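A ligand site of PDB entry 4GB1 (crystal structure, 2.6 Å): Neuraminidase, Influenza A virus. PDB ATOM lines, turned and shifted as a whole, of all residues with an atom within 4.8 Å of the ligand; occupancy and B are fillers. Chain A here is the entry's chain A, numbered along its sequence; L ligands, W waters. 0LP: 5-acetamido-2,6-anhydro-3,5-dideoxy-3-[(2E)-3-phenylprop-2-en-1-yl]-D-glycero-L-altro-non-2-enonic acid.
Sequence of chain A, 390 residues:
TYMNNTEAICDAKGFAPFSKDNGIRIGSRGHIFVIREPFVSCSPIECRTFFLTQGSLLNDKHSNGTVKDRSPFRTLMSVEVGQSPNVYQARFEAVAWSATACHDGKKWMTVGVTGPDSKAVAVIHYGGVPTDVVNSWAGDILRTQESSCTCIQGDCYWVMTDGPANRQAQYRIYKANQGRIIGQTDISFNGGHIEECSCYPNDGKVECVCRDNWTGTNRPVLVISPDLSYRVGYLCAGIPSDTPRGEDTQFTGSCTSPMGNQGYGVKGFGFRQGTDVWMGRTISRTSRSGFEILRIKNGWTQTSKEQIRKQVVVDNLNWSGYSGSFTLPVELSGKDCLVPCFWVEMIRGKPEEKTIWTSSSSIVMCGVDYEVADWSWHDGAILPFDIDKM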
ATOM      1  N   ARG A  36     -17.369   5.800   5.627  1.00  0.00           N
ATOM      2  CA  ARG A  36     -18.013   4.692   6.303  1.00  0.00           C
ATOM      3  C   ARG A  36     -18.514   3.777   5.210  1.00  0.00           C
ATOM      4  O   ARG A  36     -18.632   4.193   4.059  1.00  0.00           O
ATOM      5  CB  ARG A  36     -19.179   5.176   7.158  1.00  0.00           C
ATOM      6  CG  ARG A  36     -18.786   5.713   8.516  1.00  0.00           C
ATOM      7  CD  ARG A  36     -18.266   4.603   9.406  1.00  0.00           C
ATOM      8  NE  ARG A  36     -18.945   3.335   9.138  1.00  0.00           N
ATOM      9  CZ  ARG A  36     -19.794   2.734   9.963  1.00  0.00           C
ATOM     10  NH1 ARG A  36     -20.341   1.568   9.615  1.00  0.00           N
ATOM     11  NH2 ARG A  36     -20.077   3.288  11.138  1.00  0.00           N
ATOM     12  N   GLU A  37     -18.773   2.526   5.571  1.00  0.00           N
ATOM     13  CA  GLU A  37     -19.385   1.541   4.689  1.00  0.00           C
ATOM     14  C   GLU A  37     -18.610   1.358   3.377  1.00  0.00           C
ATOM     15  O   GLU A  37     -19.147   1.618   2.301  1.00  0.00           O
ATOM     16  CB  GLU A  37     -20.837   1.938   4.450  1.00  0.00           C
ATOM     17  CG  GLU A  37     -21.518   2.351   5.767  1.00  0.00           C
ATOM     18  CD  GLU A  37     -22.773   3.170   5.573  1.00  0.00           C
ATOM     19  OE1 GLU A  37     -23.564   2.826   4.681  1.00  0.00           O
ATOM     20  OE2 GLU A  37     -22.968   4.162   6.308  1.00  0.00           O
ATOM     21  N   GLN A  54     -18.093  11.324   3.917  1.00  0.00           N
ATOM     22  CA  GLN A  54     -18.803  12.351   4.658  1.00  0.00           C
ATOM     23  C   GLN A  54     -18.469  13.693   4.022  1.00  0.00           C
ATOM     24  O   GLN A  54     -18.824  14.750   4.530  1.00  0.00           O
ATOM     25  CB  GLN A  54     -18.392  12.302   6.126  1.00  0.00           C
ATOM     26  CG  GLN A  54     -18.408  10.890   6.706  1.00  0.00           C
ATOM     27  CD  GLN A  54     -18.244  10.870   8.215  1.00  0.00           C
ATOM     28  OE1 GLN A  54     -18.072  11.908   8.860  1.00  0.00           O
ATOM     29  NE2 GLN A  54     -18.292   9.672   8.792  1.00  0.00           N
ATOM     30  N   ASP A  69     -25.302  11.504   9.340  1.00  0.00           N
ATOM     31  CA  ASP A  69     -25.070  10.368   8.456  1.00  0.00           C
ATOM     32  C   ASP A  69     -25.702  10.737   7.122  1.00  0.00           C
ATOM     33  O   ASP A  69     -25.054  10.735   6.076  1.00  0.00           O
ATOM     34  CB  ASP A  69     -25.677   9.081   9.041  1.00  0.00           C
ATOM     35  CG  ASP A  69     -25.674   9.052  10.582  1.00  0.00           C
ATOM     36  OD1 ASP A  69     -25.162  10.006  11.208  1.00  0.00           O
ATOM     37  OD2 ASP A  69     -26.184   8.071  11.161  1.00  0.00           O
ATOM     38  N   ARG A  70     -26.981  11.097   7.173  1.00  0.00           N
ATOM     39  CA  ARG A  70     -27.770  11.348   5.983  1.00  0.00           C
ATOM     40  C   ARG A  70     -27.771  12.811   5.519  1.00  0.00           C
ATOM     41  O   ARG A  70     -28.841  13.408   5.342  1.00  0.00           O
ATOM     42  CB  ARG A  70     -29.201  10.872   6.227  1.00  0.00           C
ATOM     43  CG  ARG A  70     -29.288   9.354   6.399  1.00  0.00           C
ATOM     44  CD  ARG A  70     -30.710   8.809   6.325  1.00  0.00           C
ATOM     45  NE  ARG A  70     -31.523   9.241   7.461  1.00  0.00           N
ATOM     46  CZ  ARG A  70     -31.309   8.882   8.721  1.00  0.00           C
ATOM     47  NH1 ARG A  70     -32.120   9.332   9.679  1.00  0.00           N
ATOM     48  NH2 ARG A  70     -30.296   8.088   9.066  1.00  0.00           N
ATOM     49  N   ARG A  74     -22.888  13.920   1.622  1.00  0.00           N
ATOM     50  CA  ARG A  74     -22.501  12.511   1.652  1.00  0.00           C
ATOM     51  C   ARG A  74     -22.506  11.959   0.223  1.00  0.00           C
ATOM     52  O   ARG A  74     -23.556  11.852  -0.393  1.00  0.00           O
ATOM     53  CB  ARG A  74     -23.485  11.748   2.535  1.00  0.00           C
ATOM     54  CG  ARG A  74     -23.011  10.422   3.053  1.00  0.00           C
ATOM     55  CD  ARG A  74     -22.499  10.511   4.474  1.00  0.00           C
ATOM     56  NE  ARG A  74     -21.591   9.411   4.766  1.00  0.00           N
ATOM     57  CZ  ARG A  74     -21.942   8.254   5.318  1.00  0.00           C
ATOM     58  NH1 ARG A  74     -21.033   7.320   5.534  1.00  0.00           N
ATOM     59  NH2 ARG A  74     -23.207   8.044   5.673  1.00  0.00           N
ATOM     60  N   TRP A  97     -26.251   8.869   0.683  1.00  0.00           N
ATOM     61  CA  TRP A  97     -26.045   8.480   2.083  1.00  0.00           C
ATOM     62  C   TRP A  97     -26.447   7.006   2.291  1.00  0.00           C
ATOM     63  O   TRP A  97     -26.540   6.523   3.413  1.00  0.00           O
ATOM     64  CB  TRP A  97     -26.743   9.399   3.089  1.00  0.00           C
ATOM     65  CG  TRP A  97     -28.153   9.858   2.766  1.00  0.00           C
ATOM     66  CD1 TRP A  97     -28.532  11.127   2.438  1.00  0.00           C
ATOM     67  CD2 TRP A  97     -29.359   9.077   2.807  1.00  0.00           C
ATOM     68  NE1 TRP A  97     -29.888  11.179   2.251  1.00  0.00           N
ATOM     69  CE2 TRP A  97     -30.429   9.940   2.470  1.00  0.00           C
ATOM     70  CE3 TRP A  97     -29.648   7.738   3.061  1.00  0.00           C
ATOM     71  CZ2 TRP A  97     -31.751   9.501   2.393  1.00  0.00           C
ATOM     72  CZ3 TRP A  97     -30.959   7.297   2.983  1.00  0.00           C
ATOM     73  CH2 TRP A  97     -31.995   8.182   2.648  1.00  0.00           C
ATOM     74  N   SER A  98     -26.673   6.315   1.188  1.00  0.00           N
ATOM     75  CA  SER A  98     -26.790   4.858   1.187  1.00  0.00           C
ATOM     76  C   SER A  98     -26.604   4.412  -0.268  1.00  0.00           C
ATOM     77  O   SER A  98     -27.132   5.055  -1.184  1.00  0.00           O
ATOM     78  CB  SER A  98     -28.122   4.408   1.773  1.00  0.00           C
ATOM     79  OG  SER A  98     -28.235   2.993   1.746  1.00  0.00           O
ATOM     80  N   ILE A 141     -37.031   6.805   5.147  1.00  0.00           N
ATOM     81  CA  ILE A 141     -35.623   6.524   4.863  1.00  0.00           C
ATOM     82  C   ILE A 141     -35.264   5.420   3.882  1.00  0.00           C
ATOM     83  O   ILE A 141     -34.631   4.443   4.248  1.00  0.00           O
ATOM     84  CB  ILE A 141     -34.847   6.244   6.157  1.00  0.00           C
ATOM     85  CG1 ILE A 141     -35.185   7.297   7.212  1.00  0.00           C
ATOM     86  CG2 ILE A 141     -33.357   6.223   5.888  1.00  0.00           C
ATOM     87  CD1 ILE A 141     -34.499   7.098   8.562  1.00  0.00           C
ATOM     88  N   ARG A 143     -33.537   2.932   1.647  1.00  0.00           N
ATOM     89  CA  ARG A 143     -32.149   2.476   1.782  1.00  0.00           C
ATOM     90  C   ARG A 143     -31.892   1.171   1.030  1.00  0.00           C
ATOM     91  O   ARG A 143     -32.794   0.584   0.430  1.00  0.00           O
ATOM     92  CB  ARG A 143     -31.699   2.358   3.259  1.00  0.00           C
ATOM     93  CG  ARG A 143     -32.672   1.638   4.173  1.00  0.00           C
ATOM     94  CD  ARG A 143     -32.650   2.169   5.611  1.00  0.00           C
ATOM     95  NE  ARG A 143     -33.422   1.317   6.520  1.00  0.00           N
ATOM     96  CZ  ARG A 143     -34.736   1.430   6.740  1.00  0.00           C
ATOM     97  NH1 ARG A 143     -35.354   0.588   7.560  1.00  0.00           N
ATOM     98  NH2 ARG A 143     -35.435   2.380   6.132  1.00  0.00           N
ATOM     99  N   GLU A 146     -25.341  -1.306   0.716  1.00  0.00           N
ATOM    100  CA  GLU A 146     -23.979  -0.954   1.170  1.00  0.00           C
ATOM    101  C   GLU A 146     -22.974  -2.071   0.866  1.00  0.00           C
ATOM    102  O   GLU A 146     -22.019  -2.285   1.614  1.00  0.00           O
ATOM    103  CB  GLU A 146     -23.898  -0.599   2.676  1.00  0.00           C
ATOM    104  CG  GLU A 146     -25.151  -0.006   3.331  1.00  0.00           C
ATOM    105  CD  GLU A 146     -25.519   1.354   2.791  1.00  0.00           C
ATOM    106  OE1 GLU A 146     -24.672   1.998   2.131  1.00  0.00           O
ATOM    107  OE2 GLU A 146     -26.670   1.782   3.032  1.00  0.00           O
ATOM    108  N   ALA A 165     -36.787   1.444  11.457  1.00  0.00           N
ATOM    109  CA  ALA A 165     -35.571   0.702  11.711  1.00  0.00           C
ATOM    110  C   ALA A 165     -35.810  -0.426  12.707  1.00  0.00           C
ATOM    111  O   ALA A 165     -34.996  -1.347  12.795  1.00  0.00           O
ATOM    112  CB  ALA A 165     -34.474   1.633  12.212  1.00  0.00           C
ATOM    113  N   GLU A 195     -32.516  -5.630   6.067  1.00  0.00           N
ATOM    114  CA  GLU A 195     -31.723  -4.432   5.789  1.00  0.00           C
ATOM    115  C   GLU A 195     -30.315  -4.775   5.352  1.00  0.00           C
ATOM    116  O   GLU A 195     -29.751  -5.779   5.775  1.00  0.00           O
ATOM    117  CB  GLU A 195     -31.610  -3.565   7.039  1.00  0.00           C
ATOM    118  CG  GLU A 195     -32.907  -2.939   7.458  1.00  0.00           C
ATOM    119  CD  GLU A 195     -32.701  -1.852   8.470  1.00  0.00           C
ATOM    120  OE1 GLU A 195     -33.366  -0.807   8.321  1.00  0.00           O
ATOM    121  OE2 GLU A 195     -31.890  -2.044   9.418  1.00  0.00           O
ATOM    122  N   GLU A 196     -29.738  -3.919   4.510  1.00  0.00           N
ATOM    123  CA  GLU A 196     -28.306  -3.989   4.189  1.00  0.00           C
ATOM    124  C   GLU A 196     -27.915  -5.384   3.732  1.00  0.00           C
ATOM    125  O   GLU A 196     -27.045  -6.013   4.333  1.00  0.00           O
ATOM    126  CB  GLU A 196     -27.475  -3.609   5.430  1.00  0.00           C
ATOM    127  CG  GLU A 196     -27.272  -2.128   5.670  1.00  0.00           C
ATOM    128  CD  GLU A 196     -26.845  -1.795   7.107  1.00  0.00           C
ATOM    129  OE1 GLU A 196     -26.727  -2.748   7.914  1.00  0.00           O
ATOM    130  OE2 GLU A 196     -26.623  -0.597   7.430  1.00  0.00           O
ATOM    131  N   ARG A 211     -29.546  -8.190   7.069  1.00  0.00           N
ATOM    132  CA  ARG A 211     -29.663  -7.908   8.499  1.00  0.00           C
ATOM    133  C   ARG A 211     -31.087  -7.662   8.950  1.00  0.00           C
ATOM    134  O   ARG A 211     -31.866  -6.983   8.274  1.00  0.00           O
ATOM    135  CB  ARG A 211     -28.777  -6.673   8.749  1.00  0.00           C
ATOM    136  CG  ARG A 211     -29.089  -5.834   9.997  1.00  0.00           C
ATOM    137  CD  ARG A 211     -28.386  -4.477   9.919  1.00  0.00           C
ATOM    138  NE  ARG A 211     -28.612  -3.626  11.104  1.00  0.00           N
ATOM    139  CZ  ARG A 211     -27.969  -2.478  11.345  1.00  0.00           C
ATOM    140  NH1 ARG A 211     -28.235  -1.784  12.443  1.00  0.00           N
ATOM    141  NH2 ARG A 211     -27.048  -2.029  10.499  1.00  0.00           N
ATOM    142  N   ASN A 213     -33.035  -5.891  11.800  1.00  0.00           N
ATOM    143  CA  ASN A 213     -32.772  -4.906  12.849  1.00  0.00           C
ATOM    144  C   ASN A 213     -33.917  -4.795  13.851  1.00  0.00           C
ATOM    145  O   ASN A 213     -33.991  -3.835  14.613  1.00  0.00           O
ATOM    146  CB  ASN A 213     -32.446  -3.518  12.246  1.00  0.00           C
ATOM    147  CG  ASN A 213     -31.507  -2.699  13.126  1.00  0.00           C
ATOM    148  OD1 ASN A 213     -30.300  -2.948  13.145  1.00  0.00           O
ATOM    149  ND2 ASN A 213     -32.034  -1.712  13.836  1.00  0.00           N
ATOM    150  N   GLY A 265     -28.532  -4.438  15.324  1.00  0.00           N
ATOM    151  CA  GLY A 265     -27.918  -5.354  14.384  1.00  0.00           C
ATOM    152  C   GLY A 265     -26.687  -4.673  13.790  1.00  0.00           C
ATOM    153  O   GLY A 265     -26.297  -3.593  14.239  1.00  0.00           O
ATOM    154  N   ARG A 288     -18.973  -4.268  18.160  1.00  0.00           N
ATOM    155  CA  ARG A 288     -18.420  -4.544  16.850  1.00  0.00           C
ATOM    156  C   ARG A 288     -16.907  -4.609  16.911  1.00  0.00           C
ATOM    157  O   ARG A 288     -16.213  -3.731  16.408  1.00  0.00           O
ATOM    158  CB  ARG A 288     -18.871  -3.454  15.884  1.00  0.00           C
ATOM    159  CG  ARG A 288     -20.373  -3.197  15.942  1.00  0.00           C
ATOM    160  CD  ARG A 288     -20.821  -2.066  15.023  1.00  0.00           C
ATOM    161  NE  ARG A 288     -22.215  -2.199  14.647  1.00  0.00           N
ATOM    162  CZ  ARG A 288     -22.852  -1.376  13.827  1.00  0.00           C
ATOM    163  NH1 ARG A 288     -24.126  -1.574  13.522  1.00  0.00           N
ATOM    164  NH2 ARG A 288     -22.195  -0.349  13.292  1.00  0.00           N
ATOM    165  N   TYR A 322     -18.847  -3.380   9.749  1.00  0.00           N
ATOM    166  CA  TYR A 322     -19.575  -3.867   8.583  1.00  0.00           C
ATOM    167  C   TYR A 322     -18.814  -4.949   7.838  1.00  0.00           C
ATOM    168  O   TYR A 322     -17.587  -5.025   7.927  1.00  0.00           O
ATOM    169  CB  TYR A 322     -19.882  -2.719   7.620  1.00  0.00           C
ATOM    170  CG  TYR A 322     -21.195  -2.035   7.901  1.00  0.00           C
ATOM    171  CD1 TYR A 322     -21.640  -1.832   9.206  1.00  0.00           C
ATOM    172  CD2 TYR A 322     -22.001  -1.593   6.861  1.00  0.00           C
ATOM    173  CE1 TYR A 322     -22.827  -1.231   9.471  1.00  0.00           C
ATOM    174  CE2 TYR A 322     -23.207  -0.979   7.123  1.00  0.00           C
ATOM    175  CZ  TYR A 322     -23.607  -0.807   8.425  1.00  0.00           C
ATOM    176  OH  TYR A 322     -24.813  -0.202   8.692  1.00  0.00           O
ATOM    177  N   THR A 358     -15.297  10.007  12.977  1.00  0.00           N
ATOM    178  CA  THR A 358     -15.447   8.582  12.833  1.00  0.00           C
ATOM    179  C   THR A 358     -15.205   8.201  11.398  1.00  0.00           C
ATOM    180  O   THR A 358     -15.723   8.852  10.474  1.00  0.00           O
ATOM    181  CB  THR A 358     -16.853   8.093  13.211  1.00  0.00           C
ATOM    182  OG1 THR A 358     -17.138   8.468  14.554  1.00  0.00           O
ATOM    183  CG2 THR A 358     -16.965   6.563  13.039  1.00  0.00           C
HETATM  184  C11 0LP L   1     -29.339   4.681   5.648  1.00  0.00           C
HETATM  185  C10 0LP L   1     -28.611   4.783   6.975  1.00  0.00           C
HETATM  186  O10 0LP L   1     -28.404   5.903   7.455  1.00  0.00           O
HETATM  187  N5  0LP L   1     -28.242   3.583   7.526  1.00  0.00           N
HETATM  188  C5  0LP L   1     -27.532   3.443   8.823  1.00  0.00           C
HETATM  189  C4  0LP L   1     -25.998   3.544   8.565  1.00  0.00           C
HETATM  190  O4  0LP L   1     -25.667   4.921   8.266  1.00  0.00           O
HETATM  191  C6  0LP L   1     -27.948   2.112   9.520  1.00  0.00           C
HETATM  192  C7  0LP L   1     -29.186   2.128  10.411  1.00  0.00           C
HETATM  193  O7  0LP L   1     -29.862   3.399  10.414  1.00  0.00           O
HETATM  194  C8  0LP L   1     -30.107   0.880  10.153  1.00  0.00           C
HETATM  195  O8  0LP L   1     -29.502  -0.232   9.428  1.00  0.00           O
HETATM  196  C9  0LP L   1     -31.371   1.288   9.434  1.00  0.00           C
HETATM  197  O9  0LP L   1     -32.413   0.928  10.326  1.00  0.00           O
HETATM  198  O6  0LP L   1     -27.009   1.615  10.477  1.00  0.00           O
HETATM  199  C2  0LP L   1     -25.705   2.052  10.584  1.00  0.00           C
HETATM  200  C1  0LP L   1     -25.129   1.408  11.716  1.00  0.00           C
HETATM  201  O1B 0LP L   1     -24.061   1.833  12.255  1.00  0.00           O
HETATM  202  O1A 0LP L   1     -25.739   0.360  12.170  1.00  0.00           O
HETATM  203  C3  0LP L   1     -25.158   2.966   9.583  1.00  0.00           C
HETATM  204  CAQ 0LP L   1     -23.659   3.212   9.401  1.00  0.00           C
HETATM  205  CAI 0LP L   1     -23.078   4.487  10.021  1.00  0.00           C
HETATM  206  CAJ 0LP L   1     -22.398   5.360   9.168  1.00  0.00           C
HETATM  207  CAX 0LP L   1     -21.844   6.633   9.819  1.00  0.00           C
HETATM  208  CAN 0LP L   1     -21.114   6.545  11.032  1.00  0.00           C
HETATM  209  CAL 0LP L   1     -20.579   7.669  11.670  1.00  0.00           C
HETATM  210  CAK 0LP L   1     -20.765   8.922  11.103  1.00  0.00           C
HETATM  211  CAM 0LP L   1     -21.477   9.049   9.898  1.00  0.00           C
HETATM  212  CAO 0LP L   1     -22.015   7.903   9.262  1.00  0.00           C
HETATM  213  O   HOH W   1     -20.004  11.795  11.279  1.00  0.00           O
HETATM  214  O   HOH W   2     -26.353   3.888   5.216  1.00  0.00           O
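OE1 of Glu 195 sits at hydrogen-bond distance from O9 of the ligand (2.8 Å). The guanidinium group (NH1) of Arg 288 lies within salt-bridge range of an oxygen (O1A) of the ligand (2.9 Å). O6 of the ligand sits close to OH of Tyr 322 (3.4 Å). OE2 of Glu 37 lies close to O4 of the ligand (3.4 Å). NH2 of Arg 211 is in salt-bridge range of O1A of the ligand. An oxygen (O10) of the ligand lies within hydrogen-bond range of the guanidinium group (NH2) of Arg 70 (3.3 Å).
Arg 36 touches the ligand. NE2 of Gln 54 touches CAM of the ligand, at 3.4 Å. CB of Asp 69 touches CAO of the ligand, 3.9 Å away. NH2 of Arg 74 touches CAO of the ligand (3.8 Å). Arg 143 touches the ligand. Ala 165 touches the ligand (CB to O9, 2.9 Å). OE2 of Glu 196 touches O8 of the ligand, at 3.5 Å. Within 4 Å of the ligand: Arg 36, Glu 37, Gln 54, Asp 69, Arg 70, Arg 74, Arg 143, Ala 165, Glu 195, Glu 196, Arg 211, Arg 288 and Tyr 322. Along chain A the residues within 4 Å of the ligand span positions 36 to 322.
OE1 of Glu 195 lies within salt-bridge range of NH1 of Arg 143 (2.5 Å). O of Gly 265 is in hydrogen-bond range of NH1 of Arg 288 (3.1 Å). The backbone carbonyl oxygen of Ala 165 sits at hydrogen-bond distance from the side-chain amide nitrogen of Asn 213 (3.2 Å). The side-chain hydroxyl (OH) of Tyr 322 is in hydrogen-bond range of the guanidinium group (NH2) of Arg 211. The guanidinium group (NH1) of Arg 74 is in salt-bridge range of the side-chain carboxylate (OE2) of Glu 37. NH1 of Arg 211 sits at hydrogen-bond distance from OD1 of Asn 213 (2.5 Å). O of Thr 358 lies within hydrogen-bond range of NE2 of Gln 54. The guanidinium group (NH2) of Arg 74 sits close to the backbone carbonyl oxygen (O) of Asp 69, at 3.3 Å.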
